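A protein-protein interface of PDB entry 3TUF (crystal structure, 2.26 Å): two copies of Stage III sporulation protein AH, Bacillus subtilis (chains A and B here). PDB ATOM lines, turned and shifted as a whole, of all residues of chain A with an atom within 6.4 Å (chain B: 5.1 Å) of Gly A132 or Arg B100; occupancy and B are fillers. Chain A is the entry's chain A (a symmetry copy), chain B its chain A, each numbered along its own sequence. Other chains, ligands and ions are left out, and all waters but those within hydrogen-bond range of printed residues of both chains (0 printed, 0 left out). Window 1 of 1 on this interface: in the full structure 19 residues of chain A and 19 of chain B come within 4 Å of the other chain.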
ATOM      1  N   THR A 125     -28.363   2.331  28.014  1.00  0.00           N
ATOM      2  CA  THR A 125     -27.166   2.998  27.533  1.00  0.00           C
ATOM      3  C   THR A 125     -27.018   2.963  25.977  1.00  0.00           C
ATOM      4  O   THR A 125     -26.512   3.960  25.377  1.00  0.00           O
ATOM      5  CB  THR A 125     -25.883   2.600  28.313  1.00  0.00           C
ATOM      6  OG1 THR A 125     -25.740   1.189  28.318  1.00  0.00           O
ATOM      7  CG2 THR A 125     -25.973   3.043  29.771  1.00  0.00           C
ATOM      8  N   LEU A 127     -29.459   3.009  23.821  1.00  0.00           N
ATOM      9  CA  LEU A 127     -30.400   3.975  23.310  1.00  0.00           C
ATOM     10  C   LEU A 127     -29.772   5.363  23.256  1.00  0.00           C
ATOM     11  O   LEU A 127     -29.911   6.042  22.229  1.00  0.00           O
ATOM     12  CB  LEU A 127     -31.663   4.017  24.153  1.00  0.00           C
ATOM     13  CG  LEU A 127     -33.028   4.178  23.484  1.00  0.00           C
ATOM     14  CD1 LEU A 127     -33.765   5.033  24.416  1.00  0.00           C
ATOM     15  CD2 LEU A 127     -33.132   4.763  22.038  1.00  0.00           C
ATOM     16  N   SER A 128     -29.100   5.775  24.349  1.00  0.00           N
ATOM     17  CA  SER A 128     -28.342   7.035  24.372  1.00  0.00           C
ATOM     18  C   SER A 128     -27.371   7.176  23.257  1.00  0.00           C
ATOM     19  O   SER A 128     -27.134   8.273  22.719  1.00  0.00           O
ATOM     20  CB  SER A 128     -27.454   7.060  25.574  1.00  0.00           C
ATOM     21  OG  SER A 128     -28.280   7.142  26.691  1.00  0.00           O
ATOM     22  N   GLU A 129     -26.710   6.074  22.986  1.00  0.00           N
ATOM     23  CA  GLU A 129     -25.716   6.110  21.970  1.00  0.00           C
ATOM     24  C   GLU A 129     -26.344   6.224  20.592  1.00  0.00           C
ATOM     25  O   GLU A 129     -25.856   7.017  19.761  1.00  0.00           O
ATOM     26  CB  GLU A 129     -24.736   4.952  22.143  1.00  0.00           C
ATOM     27  CG  GLU A 129     -23.860   5.156  23.429  1.00  0.00           C
ATOM     28  CD  GLU A 129     -23.164   6.585  23.515  1.00  0.00           C
ATOM     29  OE1 GLU A 129     -22.744   7.113  22.459  1.00  0.00           O
ATOM     30  OE2 GLU A 129     -23.040   7.184  24.635  1.00  0.00           O
ATOM     31  N   VAL A 130     -27.449   5.488  20.387  1.00  0.00           N
ATOM     32  CA  VAL A 130     -28.317   5.682  19.245  1.00  0.00           C
ATOM     33  C   VAL A 130     -28.740   7.151  19.161  1.00  0.00           C
ATOM     34  O   VAL A 130     -28.576   7.795  18.105  1.00  0.00           O
ATOM     35  CB  VAL A 130     -29.570   4.755  19.357  1.00  0.00           C
ATOM     36  CG1 VAL A 130     -30.828   5.287  18.546  1.00  0.00           C
ATOM     37  CG2 VAL A 130     -29.196   3.327  18.970  1.00  0.00           C
ATOM     38  N   GLU A 131     -29.268   7.688  20.267  1.00  0.00           N
ATOM     39  CA  GLU A 131     -29.640   9.118  20.312  1.00  0.00           C
ATOM     40  C   GLU A 131     -28.488   9.998  19.819  1.00  0.00           C
ATOM     41  O   GLU A 131     -28.691  10.877  18.962  1.00  0.00           O
ATOM     42  CB  GLU A 131     -30.044   9.611  21.739  1.00  0.00           C
ATOM     43  CG  GLU A 131     -31.287   8.976  22.469  1.00  0.00           C
ATOM     44  CD  GLU A 131     -32.656   9.478  21.930  1.00  0.00           C
ATOM     45  OE1 GLU A 131     -32.650  10.322  20.982  1.00  0.00           O
ATOM     46  OE2 GLU A 131     -33.733   9.030  22.463  1.00  0.00           O
ATOM     47  N   GLY A 132     -27.293   9.762  20.381  1.00  0.00           N
ATOM     48  CA  GLY A 132     -26.102  10.555  20.036  1.00  0.00           C
ATOM     49  C   GLY A 132     -25.714  10.428  18.564  1.00  0.00           C
ATOM     50  O   GLY A 132     -25.379  11.444  17.889  1.00  0.00           O
ATOM     51  N   THR A 133     -25.765   9.173  18.077  1.00  0.00           N
ATOM     52  CA  THR A 133     -25.486   8.846  16.692  1.00  0.00           C
ATOM     53  C   THR A 133     -26.405   9.596  15.745  1.00  0.00           C
ATOM     54  O   THR A 133     -25.942  10.202  14.780  1.00  0.00           O
ATOM     55  CB  THR A 133     -25.675   7.374  16.461  1.00  0.00           C
ATOM     56  OG1 THR A 133     -24.592   6.669  17.095  1.00  0.00           O
ATOM     57  CG2 THR A 133     -25.747   7.034  14.908  1.00  0.00           C
ATOM     58  N   GLU A 134     -27.702   9.581  16.018  1.00  0.00           N
ATOM     59  CA  GLU A 134     -28.617  10.295  15.152  1.00  0.00           C
ATOM     60  C   GLU A 134     -28.418  11.813  15.098  1.00  0.00           C
ATOM     61  O   GLU A 134     -28.435  12.390  13.998  1.00  0.00           O
ATOM     62  CB  GLU A 134     -30.015  10.033  15.615  1.00  0.00           C
ATOM     63  CG  GLU A 134     -30.233   8.603  15.911  1.00  0.00           C
ATOM     64  CD  GLU A 134     -31.664   8.353  16.262  1.00  0.00           C
ATOM     65  OE1 GLU A 134     -32.339   9.344  16.637  1.00  0.00           O
ATOM     66  OE2 GLU A 134     -32.110   7.189  16.139  1.00  0.00           O
ATOM     67  N   LYS A 135     -28.274  12.454  16.281  1.00  0.00           N
ATOM     68  CA  LYS A 135     -28.020  13.903  16.379  1.00  0.00           C
ATOM     69  C   LYS A 135     -26.715  14.216  15.606  1.00  0.00           C
ATOM     70  O   LYS A 135     -26.670  15.110  14.717  1.00  0.00           O
ATOM     71  CB  LYS A 135     -27.946  14.413  17.864  1.00  0.00           C
ATOM     72  CG  LYS A 135     -29.273  14.258  18.732  1.00  0.00           C
ATOM     73  CD  LYS A 135     -29.168  14.622  20.295  1.00  0.00           C
ATOM     74  CE  LYS A 135     -29.026  16.140  20.541  1.00  0.00           C
ATOM     75  NZ  LYS A 135     -29.317  16.738  21.949  1.00  0.00           N
ATOM     76  N   GLN A 136     -25.648  13.485  15.891  1.00  0.00           N
ATOM     77  CA  GLN A 136     -24.406  13.845  15.197  1.00  0.00           C
ATOM     78  C   GLN A 136     -24.502  13.666  13.639  1.00  0.00           C
ATOM     79  O   GLN A 136     -24.016  14.530  12.805  1.00  0.00           O
ATOM     80  CB  GLN A 136     -23.227  13.075  15.781  1.00  0.00           C
ATOM     81  CG  GLN A 136     -21.880  13.688  15.464  1.00  0.00           C
ATOM     82  CD  GLN A 136     -20.815  12.631  15.392  1.00  0.00           C
ATOM     83  OE1 GLN A 136     -20.805  11.767  14.488  1.00  0.00           O
ATOM     84  NE2 GLN A 136     -19.917  12.664  16.361  1.00  0.00           N
ATOM     85  N   LEU A 137     -25.147  12.561  13.244  1.00  0.00           N
ATOM     86  CA  LEU A 137     -25.209  12.250  11.837  1.00  0.00           C
ATOM     87  C   LEU A 137     -25.949  13.402  11.116  1.00  0.00           C
ATOM     88  O   LEU A 137     -25.474  13.972  10.089  1.00  0.00           O
ATOM     89  CB  LEU A 137     -25.838  10.890  11.652  1.00  0.00           C
ATOM     90  CG  LEU A 137     -25.192   9.918  10.651  1.00  0.00           C
ATOM     91  CD1 LEU A 137     -25.021  10.649   9.352  1.00  0.00           C
ATOM     92  CD2 LEU A 137     -23.790   9.345  11.132  1.00  0.00           C
ATOM     93  N   GLU B  93     -22.426  17.606  21.516  1.00  0.00           N
ATOM     94  CA  GLU B  93     -22.451  16.158  21.358  1.00  0.00           C
ATOM     95  C   GLU B  93     -21.175  15.567  21.939  1.00  0.00           C
ATOM     96  O   GLU B  93     -21.208  14.877  22.957  1.00  0.00           O
ATOM     97  CB  GLU B  93     -22.586  15.780  19.882  1.00  0.00           C
ATOM     98  CG  GLU B  93     -23.941  15.199  19.513  1.00  0.00           C
ATOM     99  CD  GLU B  93     -25.011  15.518  20.539  1.00  0.00           C
ATOM    100  OE1 GLU B  93     -25.213  14.700  21.462  1.00  0.00           O
ATOM    101  OE2 GLU B  93     -25.649  16.584  20.422  1.00  0.00           O
ATOM    102  N   ARG B  96     -21.264  15.736  25.567  1.00  0.00           N
ATOM    103  CA  ARG B  96     -22.264  14.811  26.099  1.00  0.00           C
ATOM    104  C   ARG B  96     -21.775  13.357  26.102  1.00  0.00           C
ATOM    105  O   ARG B  96     -21.969  12.629  27.077  1.00  0.00           O
ATOM    106  CB  ARG B  96     -23.570  14.923  25.309  1.00  0.00           C
ATOM    107  CG  ARG B  96     -24.119  16.338  25.216  1.00  0.00           C
ATOM    108  CD  ARG B  96     -24.778  16.762  26.518  1.00  0.00           C
ATOM    109  NE  ARG B  96     -26.205  17.019  26.349  1.00  0.00           N
ATOM    110  CZ  ARG B  96     -26.775  18.207  26.520  1.00  0.00           C
ATOM    111  NH1 ARG B  96     -26.040  19.254  26.866  1.00  0.00           N
ATOM    112  NH2 ARG B  96     -28.082  18.349  26.346  1.00  0.00           N
ATOM    113  N   SER B  97     -21.147  12.947  25.005  1.00  0.00           N
ATOM    114  CA  SER B  97     -20.651  11.566  24.819  1.00  0.00           C
ATOM    115  C   SER B  97     -19.720  11.170  25.919  1.00  0.00           C
ATOM    116  O   SER B  97     -19.888  10.104  26.551  1.00  0.00           O
ATOM    117  CB  SER B  97     -19.815  11.461  23.568  1.00  0.00           C
ATOM    118  OG  SER B  97     -20.664  11.208  22.501  1.00  0.00           O
ATOM    119  N   LYS B  98     -18.717  12.040  26.091  1.00  0.00           N
ATOM    120  CA  LYS B  98     -17.726  11.903  27.110  1.00  0.00           C
ATOM    121  C   LYS B  98     -18.423  11.795  28.418  1.00  0.00           C
ATOM    122  O   LYS B  98     -18.147  10.864  29.189  1.00  0.00           O
ATOM    123  CB  LYS B  98     -16.802  13.114  27.146  1.00  0.00           C
ATOM    124  CG  LYS B  98     -15.571  12.922  26.297  1.00  0.00           C
ATOM    125  CD  LYS B  98     -14.829  14.289  25.983  1.00  0.00           C
ATOM    126  CE  LYS B  98     -15.290  14.943  24.629  1.00  0.00           C
ATOM    127  NZ  LYS B  98     -15.058  16.432  24.550  1.00  0.00           N
ATOM    128  N   GLU B  99     -19.326  12.745  28.678  1.00  0.00           N
ATOM    129  CA  GLU B  99     -20.154  12.650  29.873  1.00  0.00           C
ATOM    130  C   GLU B  99     -20.766  11.256  30.121  1.00  0.00           C
ATOM    131  O   GLU B  99     -20.508  10.662  31.186  1.00  0.00           O
ATOM    132  CB  GLU B  99     -21.257  13.649  29.804  1.00  0.00           C
ATOM    133  CG  GLU B  99     -20.982  14.877  30.552  1.00  0.00           C
ATOM    134  CD  GLU B  99     -22.265  15.383  31.202  1.00  0.00           C
ATOM    135  OE1 GLU B  99     -22.621  14.844  32.283  1.00  0.00           O
ATOM    136  OE2 GLU B  99     -22.925  16.286  30.626  1.00  0.00           O
ATOM    137  N   ARG B 100     -21.556  10.748  29.159  1.00  0.00           N
ATOM    138  CA  ARG B 100     -22.250   9.462  29.329  1.00  0.00           C
ATOM    139  C   ARG B 100     -21.267   8.385  29.627  1.00  0.00           C
ATOM    140  O   ARG B 100     -21.491   7.551  30.498  1.00  0.00           O
ATOM    141  CB  ARG B 100     -22.988   9.038  28.074  1.00  0.00           C
ATOM    142  CG  ARG B 100     -24.130   9.932  27.705  1.00  0.00           C
ATOM    143  CD  ARG B 100     -24.933   9.355  26.539  1.00  0.00           C
ATOM    144  NE  ARG B 100     -24.332   9.539  25.195  1.00  0.00           N
ATOM    145  CZ  ARG B 100     -24.393  10.670  24.474  1.00  0.00           C
ATOM    146  NH1 ARG B 100     -25.017  11.760  24.957  1.00  0.00           N
ATOM    147  NH2 ARG B 100     -23.832  10.705  23.274  1.00  0.00           N
ATOM    148  N   GLU B 101     -20.165   8.410  28.889  1.00  0.00           N
ATOM    149  CA  GLU B 101     -19.134   7.419  29.058  1.00  0.00           C
ATOM    150  C   GLU B 101     -18.572   7.365  30.505  1.00  0.00           C
ATOM    151  O   GLU B 101     -18.285   6.279  31.052  1.00  0.00           O
ATOM    152  CB  GLU B 101     -18.032   7.708  28.073  1.00  0.00           C
ATOM    153  CG  GLU B 101     -16.700   7.728  28.761  1.00  0.00           C
ATOM    154  CD  GLU B 101     -15.565   7.412  27.853  1.00  0.00           C
ATOM    155  OE1 GLU B 101     -15.735   7.563  26.618  1.00  0.00           O
ATOM    156  OE2 GLU B 101     -14.504   7.010  28.386  1.00  0.00           O
ATOM    157  N   GLU B 102     -18.419   8.539  31.111  1.00  0.00           N
ATOM    158  CA  GLU B 102     -17.890   8.605  32.443  1.00  0.00           C
ATOM    159  C   GLU B 102     -18.907   8.161  33.464  1.00  0.00           C
ATOM    160  O   GLU B 102     -18.595   7.328  34.342  1.00  0.00           O
ATOM    161  CB  GLU B 102     -17.388   9.992  32.730  1.00  0.00           C
ATOM    162  CG  GLU B 102     -15.913  10.121  32.402  1.00  0.00           C
ATOM    163  CD  GLU B 102     -15.522  11.495  31.861  1.00  0.00           C
ATOM    164  OE1 GLU B 102     -16.125  12.517  32.280  1.00  0.00           O
ATOM    165  OE2 GLU B 102     -14.596  11.546  31.011  1.00  0.00           O
ATOM    166  N   LEU B 103     -20.123   8.689  33.354  1.00  0.00           N
ATOM    167  CA  LEU B 103     -21.214   8.170  34.172  1.00  0.00           C
ATOM    168  C   LEU B 103     -21.268   6.635  34.060  1.00  0.00           C
ATOM    169  O   LEU B 103     -21.187   5.901  35.061  1.00  0.00           O
ATOM    170  CB  LEU B 103     -22.559   8.808  33.791  1.00  0.00           C
ATOM    171  CG  LEU B 103     -22.930  10.232  34.310  1.00  0.00           C
ATOM    172  CD1 LEU B 103     -22.036  10.707  35.480  1.00  0.00           C
ATOM    173  CD2 LEU B 103     -22.983  11.281  33.185  1.00  0.00           C
ATOM    174  N   ASN B 104     -21.341   6.135  32.839  1.00  0.00           N
ATOM    175  CA  ASN B 104     -21.423   4.706  32.695  1.00  0.00           C
ATOM    176  C   ASN B 104     -20.236   4.002  33.340  1.00  0.00           C
ATOM    177  O   ASN B 104     -20.367   2.892  33.871  1.00  0.00           O
ATOM    178  CB  ASN B 104     -21.494   4.333  31.233  1.00  0.00           C
ATOM    179  CG  ASN B 104     -21.874   2.874  31.020  1.00  0.00           C
ATOM    180  OD1 ASN B 104     -22.287   2.141  31.938  1.00  0.00           O
ATOM    181  ND2 ASN B 104     -21.741   2.447  29.791  1.00  0.00           N
ATOM    182  N   ALA B 105     -19.079   4.655  33.287  1.00  0.00           N
ATOM    183  CA  ALA B 105     -17.870   4.038  33.755  1.00  0.00           C
ATOM    184  C   ALA B 105     -17.899   3.831  35.278  1.00  0.00           C
ATOM    185  O   ALA B 105     -17.523   2.765  35.777  1.00  0.00           O
ATOM    186  CB  ALA B 105     -16.672   4.870  33.329  1.00  0.00           C
ATOM    187  N   LEU B 127     -29.627  13.372  32.403  1.00  0.00           N
ATOM    188  CA  LEU B 127     -29.026  13.839  31.177  1.00  0.00           C
ATOM    189  C   LEU B 127     -29.899  13.483  29.980  1.00  0.00           C
ATOM    190  O   LEU B 127     -30.129  14.354  29.129  1.00  0.00           O
ATOM    191  CB  LEU B 127     -27.635  13.259  30.987  1.00  0.00           C
ATOM    192  CG  LEU B 127     -26.514  14.124  30.411  1.00  0.00           C
ATOM    193  CD1 LEU B 127     -25.759  13.190  29.576  1.00  0.00           C
ATOM    194  CD2 LEU B 127     -26.855  15.410  29.590  1.00  0.00           C
ATOM    195  N   GLU B 131     -31.500  15.773  27.375  1.00  0.00           N
ATOM    196  CA  GLU B 131     -31.404  15.502  25.925  1.00  0.00           C
ATOM    197  C   GLU B 131     -32.782  15.575  25.262  1.00  0.00           C
ATOM    198  O   GLU B 131     -32.950  16.253  24.233  1.00  0.00           O
ATOM    199  CB  GLU B 131     -30.785  14.106  25.592  1.00  0.00           C
ATOM    200  CG  GLU B 131     -29.312  13.772  26.038  1.00  0.00           C
ATOM    201  CD  GLU B 131     -28.221  14.442  25.156  1.00  0.00           C
ATOM    202  OE1 GLU B 131     -28.602  15.175  24.192  1.00  0.00           O
ATOM    203  OE2 GLU B 131     -26.987  14.227  25.427  1.00  0.00           O
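OE2 of Glu B131 lies within salt-bridge range of NE of Arg B96 (3.0 Å). The guanidinium group of Arg B100 is in hydrogen-bond range of the side-chain hydroxyl of Ser B97 (3.3 Å). OE2 of Glu B131 lies within salt-bridge range of NH1 of Arg B100. The backbone carbonyl oxygen (O) of Glu A129 is in hydrogen-bond range of the side-chain hydroxyl (OG1) of Thr A133, 3.0 Å away.
Among the printed residues, pairs that only touch across the chains: Ser A128 with Arg B100 and Gly A132 with Arg B100.
The side-chain carboxylate (OE2) of Glu B93 lies within salt-bridge range of the side-chain amino group (NZ) of Lys A135 (3.98 Å). The side-chain carboxylate of Glu A129 lies within salt-bridge range of the guanidinium group of Arg B100 (2.7 Å). OE1 of Glu B131 lies within salt-bridge range of NZ of Lys A135, 2.8 Å away.
Of the 13 printed residues of chain B, 3 touch a printed residue of chain A. Printed residues of chain B that touch a printed residue of chain A: Glu B93, Arg B100 and Glu B131. Printed residues of chain A that touch a printed residue of chain B: Ser A128, Glu A129, Gly A132 and Lys A135. Among the printed residues, Asp or Glu carboxylates within 4 Å of a Lys or Arg side-chain nitrogen of the other chain: Glu A129 with Arg B100 (2.7 Å), Lys A135 with Glu B93 (3.98 Å) and Lys A135 with Glu B131 (2.8 Å).
Of the printed residues of chain B, Glu A129 touches Arg B100. Gly A132 touches just one residue of chain B: Arg B100. Of the printed residues of chain B, Lys A135 touches Glu B93 (3.4 Å) and Glu B131 (2.8 Å). Ser B97 touches none of the printed residues of chain A. Printed residues of chain A within 4 Å of Arg B100: Ser A128 (3.5 Å), Glu A129 (2.7 Å) and Gly A132 (3.96 Å). Ala B105 touches none of the printed residues of chain A. Of the printed residues of chain A, Glu B131 touches Lys A135 (2.8 Å). The nearest printed residue of chain A that does not touch Arg B100 is Thr A125 (5.7 Å).
2 positions are printed for both chains. Of the 5 pairs that touch across the chains among the printed residues, none has its exchanged pair printed and touching as well.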
